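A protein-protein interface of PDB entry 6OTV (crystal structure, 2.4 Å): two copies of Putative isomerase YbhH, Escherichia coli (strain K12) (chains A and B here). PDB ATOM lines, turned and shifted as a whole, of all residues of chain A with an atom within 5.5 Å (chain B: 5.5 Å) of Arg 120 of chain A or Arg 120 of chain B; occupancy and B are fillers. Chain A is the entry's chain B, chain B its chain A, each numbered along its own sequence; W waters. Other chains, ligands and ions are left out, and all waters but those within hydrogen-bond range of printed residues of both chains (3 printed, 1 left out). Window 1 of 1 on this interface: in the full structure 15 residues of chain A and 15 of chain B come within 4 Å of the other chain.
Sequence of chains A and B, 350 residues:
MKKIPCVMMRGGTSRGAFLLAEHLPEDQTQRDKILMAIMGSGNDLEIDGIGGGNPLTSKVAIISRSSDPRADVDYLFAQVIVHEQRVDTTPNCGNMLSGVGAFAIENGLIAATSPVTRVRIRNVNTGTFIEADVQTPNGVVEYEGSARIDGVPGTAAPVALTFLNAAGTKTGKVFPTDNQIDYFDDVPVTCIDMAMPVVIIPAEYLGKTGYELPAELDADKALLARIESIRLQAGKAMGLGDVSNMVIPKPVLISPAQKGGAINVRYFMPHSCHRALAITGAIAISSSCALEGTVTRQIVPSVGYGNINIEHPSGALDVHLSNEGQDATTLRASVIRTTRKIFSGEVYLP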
ATOM      1  N   PRO A  69     -16.024  14.673  23.114  1.00  0.00           N
ATOM      2  CA  PRO A  69     -16.175  15.702  24.155  1.00  0.00           C
ATOM      3  C   PRO A  69     -15.196  16.859  24.026  1.00  0.00           C
ATOM      4  O   PRO A  69     -15.413  17.901  24.659  1.00  0.00           O
ATOM      5  CB  PRO A  69     -15.945  14.923  25.457  1.00  0.00           C
ATOM      6  CG  PRO A  69     -15.145  13.724  25.048  1.00  0.00           C
ATOM      7  CD  PRO A  69     -15.617  13.371  23.670  1.00  0.00           C
ATOM      8  N   ARG A  70     -14.141  16.720  23.227  1.00  0.00           N
ATOM      9  CA  ARG A  70     -13.158  17.778  23.064  1.00  0.00           C
ATOM     10  C   ARG A  70     -13.531  18.789  21.987  1.00  0.00           C
ATOM     11  O   ARG A  70     -12.878  19.834  21.894  1.00  0.00           O
ATOM     12  CB  ARG A  70     -11.786  17.172  22.746  1.00  0.00           C
ATOM     13  CG  ARG A  70     -11.220  16.323  23.874  1.00  0.00           C
ATOM     14  CD  ARG A  70     -10.117  15.404  23.381  1.00  0.00           C
ATOM     15  NE  ARG A  70     -10.611  14.459  22.385  1.00  0.00           N
ATOM     16  CZ  ARG A  70      -9.865  13.519  21.812  1.00  0.00           C
ATOM     17  NH1 ARG A  70      -8.586  13.395  22.138  1.00  0.00           N
ATOM     18  NH2 ARG A  70     -10.401  12.702  20.914  1.00  0.00           N
ATOM     19  N   ALA A  71     -14.558  18.519  21.184  1.00  0.00           N
ATOM     20  CA  ALA A  71     -14.948  19.413  20.104  1.00  0.00           C
ATOM     21  C   ALA A  71     -16.382  19.889  20.298  1.00  0.00           C
ATOM     22  O   ALA A  71     -17.166  19.291  21.041  1.00  0.00           O
ATOM     23  CB  ALA A  71     -14.807  18.731  18.737  1.00  0.00           C
ATOM     24  N   ASP A  72     -16.718  20.985  19.619  1.00  0.00           N
ATOM     25  CA  ASP A  72     -18.086  21.485  19.608  1.00  0.00           C
ATOM     26  C   ASP A  72     -18.894  20.859  18.478  1.00  0.00           C
ATOM     27  O   ASP A  72     -20.000  20.361  18.702  1.00  0.00           O
ATOM     28  CB  ASP A  72     -18.100  23.013  19.479  1.00  0.00           C
ATOM     29  CG  ASP A  72     -17.284  23.705  20.560  1.00  0.00           C
ATOM     30  OD1 ASP A  72     -17.300  23.240  21.719  1.00  0.00           O
ATOM     31  OD2 ASP A  72     -16.621  24.717  20.248  1.00  0.00           O
ATOM     32  N   VAL A  73     -18.357  20.871  17.260  1.00  0.00           N
ATOM     33  CA  VAL A  73     -19.066  20.348  16.102  1.00  0.00           C
ATOM     34  C   VAL A  73     -18.175  19.363  15.362  1.00  0.00           C
ATOM     35  O   VAL A  73     -16.943  19.451  15.402  1.00  0.00           O
ATOM     36  CB  VAL A  73     -19.535  21.469  15.146  1.00  0.00           C
ATOM     37  CG1 VAL A  73     -20.402  22.474  15.882  1.00  0.00           C
ATOM     38  CG2 VAL A  73     -18.348  22.156  14.501  1.00  0.00           C
ATOM     39  N   ILE A 110     -24.043  25.860  18.405  1.00  0.00           N
ATOM     40  CA  ILE A 110     -23.197  26.403  19.461  1.00  0.00           C
ATOM     41  C   ILE A 110     -23.634  27.838  19.717  1.00  0.00           C
ATOM     42  O   ILE A 110     -24.019  28.559  18.792  1.00  0.00           O
ATOM     43  CB  ILE A 110     -21.698  26.311  19.084  1.00  0.00           C
ATOM     44  CG1 ILE A 110     -20.823  26.938  20.173  1.00  0.00           C
ATOM     45  CG2 ILE A 110     -21.438  26.961  17.732  1.00  0.00           C
ATOM     46  CD1 ILE A 110     -19.347  26.887  19.871  1.00  0.00           C
ATOM     47  N   ARG A 118     -15.531  31.340  19.468  1.00  0.00           N
ATOM     48  CA  ARG A 118     -14.639  30.214  19.234  1.00  0.00           C
ATOM     49  C   ARG A 118     -15.458  28.965  18.936  1.00  0.00           C
ATOM     50  O   ARG A 118     -16.445  28.682  19.623  1.00  0.00           O
ATOM     51  CB  ARG A 118     -13.743  29.982  20.451  1.00  0.00           C
ATOM     52  CG  ARG A 118     -12.951  31.203  20.883  1.00  0.00           C
ATOM     53  CD  ARG A 118     -12.179  30.944  22.171  1.00  0.00           C
ATOM     54  NE  ARG A 118     -11.038  30.054  21.974  1.00  0.00           N
ATOM     55  CZ  ARG A 118     -10.195  29.695  22.937  1.00  0.00           C
ATOM     56  NH1 ARG A 118     -10.366  30.146  24.173  1.00  0.00           N
ATOM     57  NH2 ARG A 118      -9.179  28.883  22.665  1.00  0.00           N
ATOM     58  N   VAL A 119     -15.056  28.222  17.906  1.00  0.00           N
ATOM     59  CA  VAL A 119     -15.727  26.983  17.528  1.00  0.00           C
ATOM     60  C   VAL A 119     -14.675  25.889  17.421  1.00  0.00           C
ATOM     61  O   VAL A 119     -13.759  25.983  16.597  1.00  0.00           O
ATOM     62  CB  VAL A 119     -16.504  27.112  16.206  1.00  0.00           C
ATOM     63  CG1 VAL A 119     -17.287  25.832  15.938  1.00  0.00           C
ATOM     64  CG2 VAL A 119     -17.435  28.317  16.236  1.00  0.00           C
ATOM     65  N   ARG A 120     -14.814  24.854  18.242  1.00  0.00           N
ATOM     66  CA  ARG A 120     -13.927  23.698  18.206  1.00  0.00           C
ATOM     67  C   ARG A 120     -14.468  22.685  17.203  1.00  0.00           C
ATOM     68  O   ARG A 120     -15.560  22.139  17.392  1.00  0.00           O
ATOM     69  CB  ARG A 120     -13.807  23.081  19.596  1.00  0.00           C
ATOM     70  CG  ARG A 120     -13.004  23.931  20.561  1.00  0.00           C
ATOM     71  CD  ARG A 120     -11.538  23.565  20.484  1.00  0.00           C
ATOM     72  NE  ARG A 120     -10.680  24.599  21.045  1.00  0.00           N
ATOM     73  CZ  ARG A 120      -9.506  24.361  21.618  1.00  0.00           C
ATOM     74  NH1 ARG A 120      -9.057  23.118  21.719  1.00  0.00           N
ATOM     75  NH2 ARG A 120      -8.787  25.365  22.097  1.00  0.00           N
ATOM     76  N   ILE A 121     -13.704  22.436  16.145  1.00  0.00           N
ATOM     77  CA  ILE A 121     -14.142  21.609  15.026  1.00  0.00           C
ATOM     78  C   ILE A 121     -13.295  20.347  14.989  1.00  0.00           C
ATOM     79  O   ILE A 121     -12.062  20.417  15.046  1.00  0.00           O
ATOM     80  CB  ILE A 121     -14.039  22.371  13.694  1.00  0.00           C
ATOM     81  CG1 ILE A 121     -14.925  23.620  13.723  1.00  0.00           C
ATOM     82  CG2 ILE A 121     -14.398  21.459  12.529  1.00  0.00           C
ATOM     83  CD1 ILE A 121     -14.655  24.581  12.586  1.00  0.00           C
ATOM     84  N   ARG A 122     -13.954  19.197  14.893  1.00  0.00           N
ATOM     85  CA  ARG A 122     -13.284  17.927  14.656  1.00  0.00           C
ATOM     86  C   ARG A 122     -13.593  17.479  13.234  1.00  0.00           C
ATOM     87  O   ARG A 122     -14.763  17.288  12.883  1.00  0.00           O
ATOM     88  CB  ARG A 122     -13.729  16.869  15.664  1.00  0.00           C
ATOM     89  CG  ARG A 122     -13.340  15.452  15.280  1.00  0.00           C
ATOM     90  CD  ARG A 122     -13.843  14.454  16.310  1.00  0.00           C
ATOM     91  NE  ARG A 122     -13.909  13.098  15.779  1.00  0.00           N
ATOM     92  CZ  ARG A 122     -15.039  12.447  15.527  1.00  0.00           C
ATOM     93  NH1 ARG A 122     -16.206  13.022  15.769  1.00  0.00           N
ATOM     94  NH2 ARG A 122     -15.002  11.214  15.041  1.00  0.00           N
ATOM     95  N   ILE A 130      -9.560  21.432  14.796  1.00  0.00           N
ATOM     96  CA  ILE A 130      -9.264  22.790  14.353  1.00  0.00           C
ATOM     97  C   ILE A 130     -10.163  23.754  15.113  1.00  0.00           C
ATOM     98  O   ILE A 130     -11.367  23.509  15.247  1.00  0.00           O
ATOM     99  CB  ILE A 130      -9.467  22.964  12.834  1.00  0.00           C
ATOM    100  CG1 ILE A 130      -8.649  21.939  12.045  1.00  0.00           C
ATOM    101  CG2 ILE A 130      -9.103  24.379  12.404  1.00  0.00           C
ATOM    102  CD1 ILE A 130      -9.455  20.740  11.591  1.00  0.00           C
ATOM    103  N   GLU A 131      -9.585  24.846  15.602  1.00  0.00           N
ATOM    104  CA  GLU A 131     -10.373  25.926  16.180  1.00  0.00           C
ATOM    105  C   GLU A 131     -10.629  26.988  15.120  1.00  0.00           C
ATOM    106  O   GLU A 131      -9.703  27.418  14.422  1.00  0.00           O
ATOM    107  CB  GLU A 131      -9.675  26.549  17.390  1.00  0.00           C
ATOM    108  CG  GLU A 131     -10.367  27.820  17.875  1.00  0.00           C
ATOM    109  CD  GLU A 131      -9.907  28.279  19.246  1.00  0.00           C
ATOM    110  OE1 GLU A 131      -9.345  27.456  20.002  1.00  0.00           O
ATOM    111  OE2 GLU A 131     -10.115  29.468  19.570  1.00  0.00           O
ATOM    112  N   ALA A 132     -11.884  27.402  14.995  1.00  0.00           N
ATOM    113  CA  ALA A 132     -12.270  28.495  14.118  1.00  0.00           C
ATOM    114  C   ALA A 132     -12.700  29.680  14.970  1.00  0.00           C
ATOM    115  O   ALA A 132     -13.479  29.520  15.916  1.00  0.00           O
ATOM    116  CB  ALA A 132     -13.400  28.079  13.173  1.00  0.00           C
ATOM    117  N   LEU A 164      -4.846  22.107  15.772  1.00  0.00           N
ATOM    118  CA  LEU A 164      -4.533  21.795  17.160  1.00  0.00           C
ATOM    119  C   LEU A 164      -3.722  20.517  17.348  1.00  0.00           C
ATOM    120  O   LEU A 164      -3.011  20.405  18.352  1.00  0.00           O
ATOM    121  CB  LEU A 164      -5.829  21.688  17.973  1.00  0.00           C
ATOM    122  CG  LEU A 164      -6.761  22.892  17.833  1.00  0.00           C
ATOM    123  CD1 LEU A 164      -8.068  22.665  18.575  1.00  0.00           C
ATOM    124  CD2 LEU A 164      -6.070  24.156  18.319  1.00  0.00           C
ATOM    125  N   PRO B  69      -0.609  23.111  22.257  1.00  0.00           N
ATOM    126  CA  PRO B  69      -1.436  23.877  21.311  1.00  0.00           C
ATOM    127  C   PRO B  69      -2.932  23.662  21.484  1.00  0.00           C
ATOM    128  O   PRO B  69      -3.717  24.451  20.943  1.00  0.00           O
ATOM    129  CB  PRO B  69      -0.960  23.374  19.941  1.00  0.00           C
ATOM    130  CG  PRO B  69      -0.369  22.026  20.217  1.00  0.00           C
ATOM    131  CD  PRO B  69       0.245  22.121  21.579  1.00  0.00           C
ATOM    132  N   ARG B  70      -3.350  22.637  22.222  1.00  0.00           N
ATOM    133  CA  ARG B  70      -4.764  22.358  22.420  1.00  0.00           C
ATOM    134  C   ARG B  70      -5.379  23.141  23.574  1.00  0.00           C
ATOM    135  O   ARG B  70      -6.609  23.157  23.701  1.00  0.00           O
ATOM    136  CB  ARG B  70      -4.970  20.856  22.647  1.00  0.00           C
ATOM    137  CG  ARG B  70      -4.585  20.007  21.444  1.00  0.00           C
ATOM    138  CD  ARG B  70      -4.438  18.541  21.810  1.00  0.00           C
ATOM    139  NE  ARG B  70      -3.346  18.328  22.754  1.00  0.00           N
ATOM    140  CZ  ARG B  70      -2.945  17.134  23.175  1.00  0.00           C
ATOM    141  NH1 ARG B  70      -3.545  16.036  22.734  1.00  0.00           N
ATOM    142  NH2 ARG B  70      -1.940  17.038  24.037  1.00  0.00           N
ATOM    143  N   ALA B  71      -4.571  23.795  24.403  1.00  0.00           N
ATOM    144  CA  ALA B  71      -5.069  24.510  25.568  1.00  0.00           C
ATOM    145  C   ALA B  71      -4.686  25.983  25.491  1.00  0.00           C
ATOM    146  O   ALA B  71      -3.780  26.375  24.752  1.00  0.00           O
ATOM    147  CB  ALA B  71      -4.530  23.900  26.868  1.00  0.00           C
ATOM    148  N   ASP B  72      -5.395  26.801  26.269  1.00  0.00           N
ATOM    149  CA  ASP B  72      -5.065  28.217  26.382  1.00  0.00           C
ATOM    150  C   ASP B  72      -4.052  28.463  27.494  1.00  0.00           C
ATOM    151  O   ASP B  72      -3.028  29.117  27.274  1.00  0.00           O
ATOM    152  CB  ASP B  72      -6.332  29.045  26.630  1.00  0.00           C
ATOM    153  CG  ASP B  72      -7.400  28.820  25.572  1.00  0.00           C
ATOM    154  OD1 ASP B  72      -7.048  28.622  24.390  1.00  0.00           O
ATOM    155  OD2 ASP B  72      -8.597  28.836  25.925  1.00  0.00           O
ATOM    156  N   VAL B  73      -4.315  27.943  28.690  1.00  0.00           N
ATOM    157  CA  VAL B  73      -3.432  28.154  29.826  1.00  0.00           C
ATOM    158  C   VAL B  73      -3.057  26.811  30.430  1.00  0.00           C
ATOM    159  O   VAL B  73      -3.798  25.827  30.330  1.00  0.00           O
ATOM    160  CB  VAL B  73      -4.065  29.069  30.900  1.00  0.00           C
ATOM    161  CG1 VAL B  73      -4.450  30.411  30.303  1.00  0.00           C
ATOM    162  CG2 VAL B  73      -5.265  28.398  31.540  1.00  0.00           C
ATOM    163  N   ILE B 110      -5.475  35.455  28.204  1.00  0.00           N
ATOM    164  CA  ILE B 110      -6.437  35.142  27.154  1.00  0.00           C
ATOM    165  C   ILE B 110      -7.403  36.314  27.045  1.00  0.00           C
ATOM    166  O   ILE B 110      -7.735  36.958  28.045  1.00  0.00           O
ATOM    167  CB  ILE B 110      -7.171  33.809  27.438  1.00  0.00           C
ATOM    168  CG1 ILE B 110      -8.201  33.510  26.345  1.00  0.00           C
ATOM    169  CG2 ILE B 110      -7.823  33.831  28.818  1.00  0.00           C
ATOM    170  CD1 ILE B 110      -8.973  32.231  26.566  1.00  0.00           C
ATOM    171  N   ARG B 118     -14.689  31.397  27.201  1.00  0.00           N
ATOM    172  CA  ARG B 118     -14.229  30.019  27.300  1.00  0.00           C
ATOM    173  C   ARG B 118     -12.723  30.000  27.522  1.00  0.00           C
ATOM    174  O   ARG B 118     -11.980  30.716  26.842  1.00  0.00           O
ATOM    175  CB  ARG B 118     -14.588  29.247  26.030  1.00  0.00           C
ATOM    176  CG  ARG B 118     -16.066  29.284  25.676  1.00  0.00           C
ATOM    177  CD  ARG B 118     -16.343  28.612  24.338  1.00  0.00           C
ATOM    178  NE  ARG B 118     -16.187  27.161  24.397  1.00  0.00           N
ATOM    179  CZ  ARG B 118     -16.362  26.347  23.361  1.00  0.00           C
ATOM    180  NH1 ARG B 118     -16.695  26.841  22.174  1.00  0.00           N
ATOM    181  NH2 ARG B 118     -16.204  25.037  23.510  1.00  0.00           N
ATOM    182  N   VAL B 119     -12.271  29.188  28.477  1.00  0.00           N
ATOM    183  CA  VAL B 119     -10.852  29.052  28.783  1.00  0.00           C
ATOM    184  C   VAL B 119     -10.499  27.572  28.763  1.00  0.00           C
ATOM    185  O   VAL B 119     -11.033  26.794  29.560  1.00  0.00           O
ATOM    186  CB  VAL B 119     -10.483  29.671  30.142  1.00  0.00           C
ATOM    187  CG1 VAL B 119      -8.980  29.565  30.370  1.00  0.00           C
ATOM    188  CG2 VAL B 119     -10.944  31.120  30.222  1.00  0.00           C
ATOM    189  N   ARG B 120      -9.598  27.188  27.864  1.00  0.00           N
ATOM    190  CA  ARG B 120      -9.123  25.812  27.771  1.00  0.00           C
ATOM    191  C   ARG B 120      -7.928  25.629  28.699  1.00  0.00           C
ATOM    192  O   ARG B 120      -6.874  26.243  28.496  1.00  0.00           O
ATOM    193  CB  ARG B 120      -8.749  25.478  26.329  1.00  0.00           C
ATOM    194  CG  ARG B 120      -9.951  25.313  25.423  1.00  0.00           C
ATOM    195  CD  ARG B 120     -10.440  23.881  25.450  1.00  0.00           C
ATOM    196  NE  ARG B 120     -11.778  23.749  24.892  1.00  0.00           N
ATOM    197  CZ  ARG B 120     -12.204  22.679  24.230  1.00  0.00           C
ATOM    198  NH1 ARG B 120     -11.385  21.655  24.029  1.00  0.00           N
ATOM    199  NH2 ARG B 120     -13.443  22.640  23.760  1.00  0.00           N
ATOM    200  N   ILE B 121      -8.090  24.781  29.710  1.00  0.00           N
ATOM    201  CA  ILE B 121      -7.103  24.609  30.769  1.00  0.00           C
ATOM    202  C   ILE B 121      -6.501  23.217  30.661  1.00  0.00           C
ATOM    203  O   ILE B 121      -7.231  22.226  30.532  1.00  0.00           O
ATOM    204  CB  ILE B 121      -7.732  24.821  32.157  1.00  0.00           C
ATOM    205  CG1 ILE B 121      -8.305  26.235  32.274  1.00  0.00           C
ATOM    206  CG2 ILE B 121      -6.714  24.543  33.258  1.00  0.00           C
ATOM    207  CD1 ILE B 121      -9.175  26.436  33.498  1.00  0.00           C
ATOM    208  N   ARG B 122      -5.177  23.140  30.715  1.00  0.00           N
ATOM    209  CA  ARG B 122      -4.467  21.874  30.822  1.00  0.00           C
ATOM    210  C   ARG B 122      -3.865  21.779  32.217  1.00  0.00           C
ATOM    211  O   ARG B 122      -3.039  22.617  32.598  1.00  0.00           O
ATOM    212  CB  ARG B 122      -3.378  21.757  29.757  1.00  0.00           C
ATOM    213  CG  ARG B 122      -2.393  20.623  30.005  1.00  0.00           C
ATOM    214  CD  ARG B 122      -1.328  20.576  28.922  1.00  0.00           C
ATOM    215  NE  ARG B 122      -0.127  19.868  29.355  1.00  0.00           N
ATOM    216  CZ  ARG B 122       1.041  20.452  29.595  1.00  0.00           C
ATOM    217  NH1 ARG B 122       1.178  21.759  29.436  1.00  0.00           N
ATOM    218  NH2 ARG B 122       2.079  19.728  29.988  1.00  0.00           N
ATOM    219  N   ILE B 130      -9.447  20.646  30.810  1.00  0.00           N
ATOM    220  CA  ILE B 130     -10.721  21.108  31.349  1.00  0.00           C
ATOM    221  C   ILE B 130     -11.068  22.437  30.698  1.00  0.00           C
ATOM    222  O   ILE B 130     -10.202  23.304  30.534  1.00  0.00           O
ATOM    223  CB  ILE B 130     -10.681  21.262  32.887  1.00  0.00           C
ATOM    224  CG1 ILE B 130     -10.187  19.977  33.558  1.00  0.00           C
ATOM    225  CG2 ILE B 130     -12.056  21.637  33.424  1.00  0.00           C
ATOM    226  CD1 ILE B 130      -8.716  20.002  33.909  1.00  0.00           C
ATOM    227  N   GLU B 131     -12.333  22.601  30.322  1.00  0.00           N
ATOM    228  CA  GLU B 131     -12.830  23.886  29.853  1.00  0.00           C
ATOM    229  C   GLU B 131     -13.547  24.592  30.996  1.00  0.00           C
ATOM    230  O   GLU B 131     -14.390  23.994  31.671  1.00  0.00           O
ATOM    231  CB  GLU B 131     -13.773  23.734  28.658  1.00  0.00           C
ATOM    232  CG  GLU B 131     -14.445  25.050  28.276  1.00  0.00           C
ATOM    233  CD  GLU B 131     -15.182  24.996  26.950  1.00  0.00           C
ATOM    234  OE1 GLU B 131     -14.860  24.130  26.108  1.00  0.00           O
ATOM    235  OE2 GLU B 131     -16.086  25.836  26.749  1.00  0.00           O
ATOM    236  N   ALA B 132     -13.199  25.856  31.213  1.00  0.00           N
ATOM    237  CA  ALA B 132     -13.872  26.708  32.182  1.00  0.00           C
ATOM    238  C   ALA B 132     -14.644  27.787  31.438  1.00  0.00           C
ATOM    239  O   ALA B 132     -14.098  28.447  30.548  1.00  0.00           O
ATOM    240  CB  ALA B 132     -12.874  27.342  33.153  1.00  0.00           C
ATOM    241  N   LEU B 164     -12.593  17.126  29.703  1.00  0.00           N
ATOM    242  CA  LEU B 164     -12.556  16.830  28.275  1.00  0.00           C
ATOM    243  C   LEU B 164     -11.958  15.471  27.936  1.00  0.00           C
ATOM    244  O   LEU B 164     -12.321  14.893  26.906  1.00  0.00           O
ATOM    245  CB  LEU B 164     -11.771  17.922  27.540  1.00  0.00           C
ATOM    246  CG  LEU B 164     -12.261  19.347  27.805  1.00  0.00           C
ATOM    247  CD1 LEU B 164     -11.354  20.371  27.141  1.00  0.00           C
ATOM    248  CD2 LEU B 164     -13.702  19.511  27.342  1.00  0.00           C
HETATM  249  O   HOH W   1     -17.706  29.746  21.630  1.00  0.00           O
HETATM  250  O   HOH W   2     -12.283  32.463  24.998  1.00  0.00           O
HETATM  251  O   HOH W   3      -6.663  26.370  22.733  1.00  0.00           O
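Among the printed residues, pairs that only touch across the chains: Pro 69 of chain A with Leu 164 of chain B, Arg 70 of chain A with Leu 164 of chain B, Ile 110 of chain A with Arg 118 of chain B, Arg 118 of chain A with Ile 110 of chain B, Arg 120 of chain A with Arg 120 of chain B, Leu 164 of chain A with Pro 69 of chain B and Leu 164 of chain A with Arg 70 of chain B.
N of Val 73 of chain B sits at hydrogen-bond distance from O of Arg 120 of chain B, at 3.1 Å.
The guanidinium group of Arg 118 of chain B lies within salt-bridge range of the side-chain carboxylate of Glu 131 of chain B (2.7 Å).
The side-chain carboxylate of Glu 131 of chain B lies within salt-bridge range of the guanidinium group of Arg 120 of chain B, at 3.1 Å.
The side-chain carboxylate (OD2) of Asp 72 of chain A sits at hydrogen-bond distance from the backbone NH (N) of Arg 120 of chain A (2.7 Å).
The backbone NH of Val 73 of chain A sits at hydrogen-bond distance from the backbone carbonyl oxygen of Arg 120 of chain A (3.1 Å).
The guanidinium group of Arg 118 of chain A is in salt-bridge range of the side-chain carboxylate of Glu 131 of chain A (2.6 Å).
Arg 70 of chain A touches Arg 120 of chain B, and with the chains exchanged Arg 120 of chain A touches Arg 70 of chain B.
Arg 70 of chain A touches Leu 164 of chain B, and with the chains exchanged Leu 164 of chain A touches Arg 70 of chain B.
Ile 110 of chain A touches Arg 118 of chain B, and with the chains exchanged Arg 118 of chain A touches Ile 110 of chain B.
Arg 120 of chain B touches its own counterpart, Arg 120 of chain A.
Of the 12 pairs that touch across the chains among the printed residues, 12 have their exchanged pair printed and touching as well.
Of the 15 printed residues of chain A, 7 touch a printed residue of chain B.
Hydrophobic or aromatic side chains of chain B that line the printed part of chain A: Pro 69, Ile 110 and Leu 164.
Among the printed residues, 12 pairs touch across the chains.
Water W3 lies within hydrogen-bond range of NH2 of Arg 120 of chain A (2.4 Å), OD1 of Asp 72 of chain B (2.8 Å) and O of Arg 70 of chain B (3.4 Å).
Water W2 bridges O of Arg 118 of chain B and NH1 of Arg 118 of chain A.
Water W1 lies within hydrogen-bond range of the backbone carbonyl oxygen (O) of Arg 118 of chain A (2.6 Å) and the guanidinium group (NH1) of Arg 118 of chain B (3.1 Å).
Arg 120 of chain A touches just these residues of chain B: Arg 70 (3.2 Å) and Arg 120 (3.5 Å).
Of chain A, only Arg 70 (3.2 Å) and Arg 120 (3.5 Å) come within 4 Å of Arg 120 of chain B.
Of the printed residues of chain A, Ile 110 of chain B touches Arg 118.
Printed residues of chain A within 4 Å of Pro 69 of chain B: Leu 164 (3.5 Å).
Of the printed residues of chain B, Pro 69 of chain A touches Leu 164 (3.6 Å).
Printed residues of chain B within 4 Å of Arg 118 of chain A: Asp 72 (2.8 Å), Ile 110 (3.5 Å) and Arg 118 (3.2 Å).
Val 119 of chain A touches none of the printed residues of chain B.
Arg 122 of chain B touches none of the printed residues of chain A.
The nearest residue of chain B that does not touch Arg 120 of chain A is Asp 72 of chain B (4.3 Å).
The backbone carbonyl oxygen of Arg 70 of chain B sits at hydrogen-bond distance from the guanidinium group of Arg 120 of chain A, at 3.2 Å.
OD1 of Asp 72 of chain B is in salt-bridge range of NH2 of Arg 118 of chain A (2.8 Å).
NH2 of Arg 118 of chain B lies within salt-bridge range of OD1 of Asp 72 of chain A (2.8 Å).
O of Arg 118 of chain A sits at hydrogen-bond distance from NH1 of Arg 118 of chain B (3.2 Å).
The guanidinium group (NH1) of Arg 120 of chain B sits at hydrogen-bond distance from the backbone carbonyl oxygen (O) of Arg 70 of chain A (3.2 Å).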
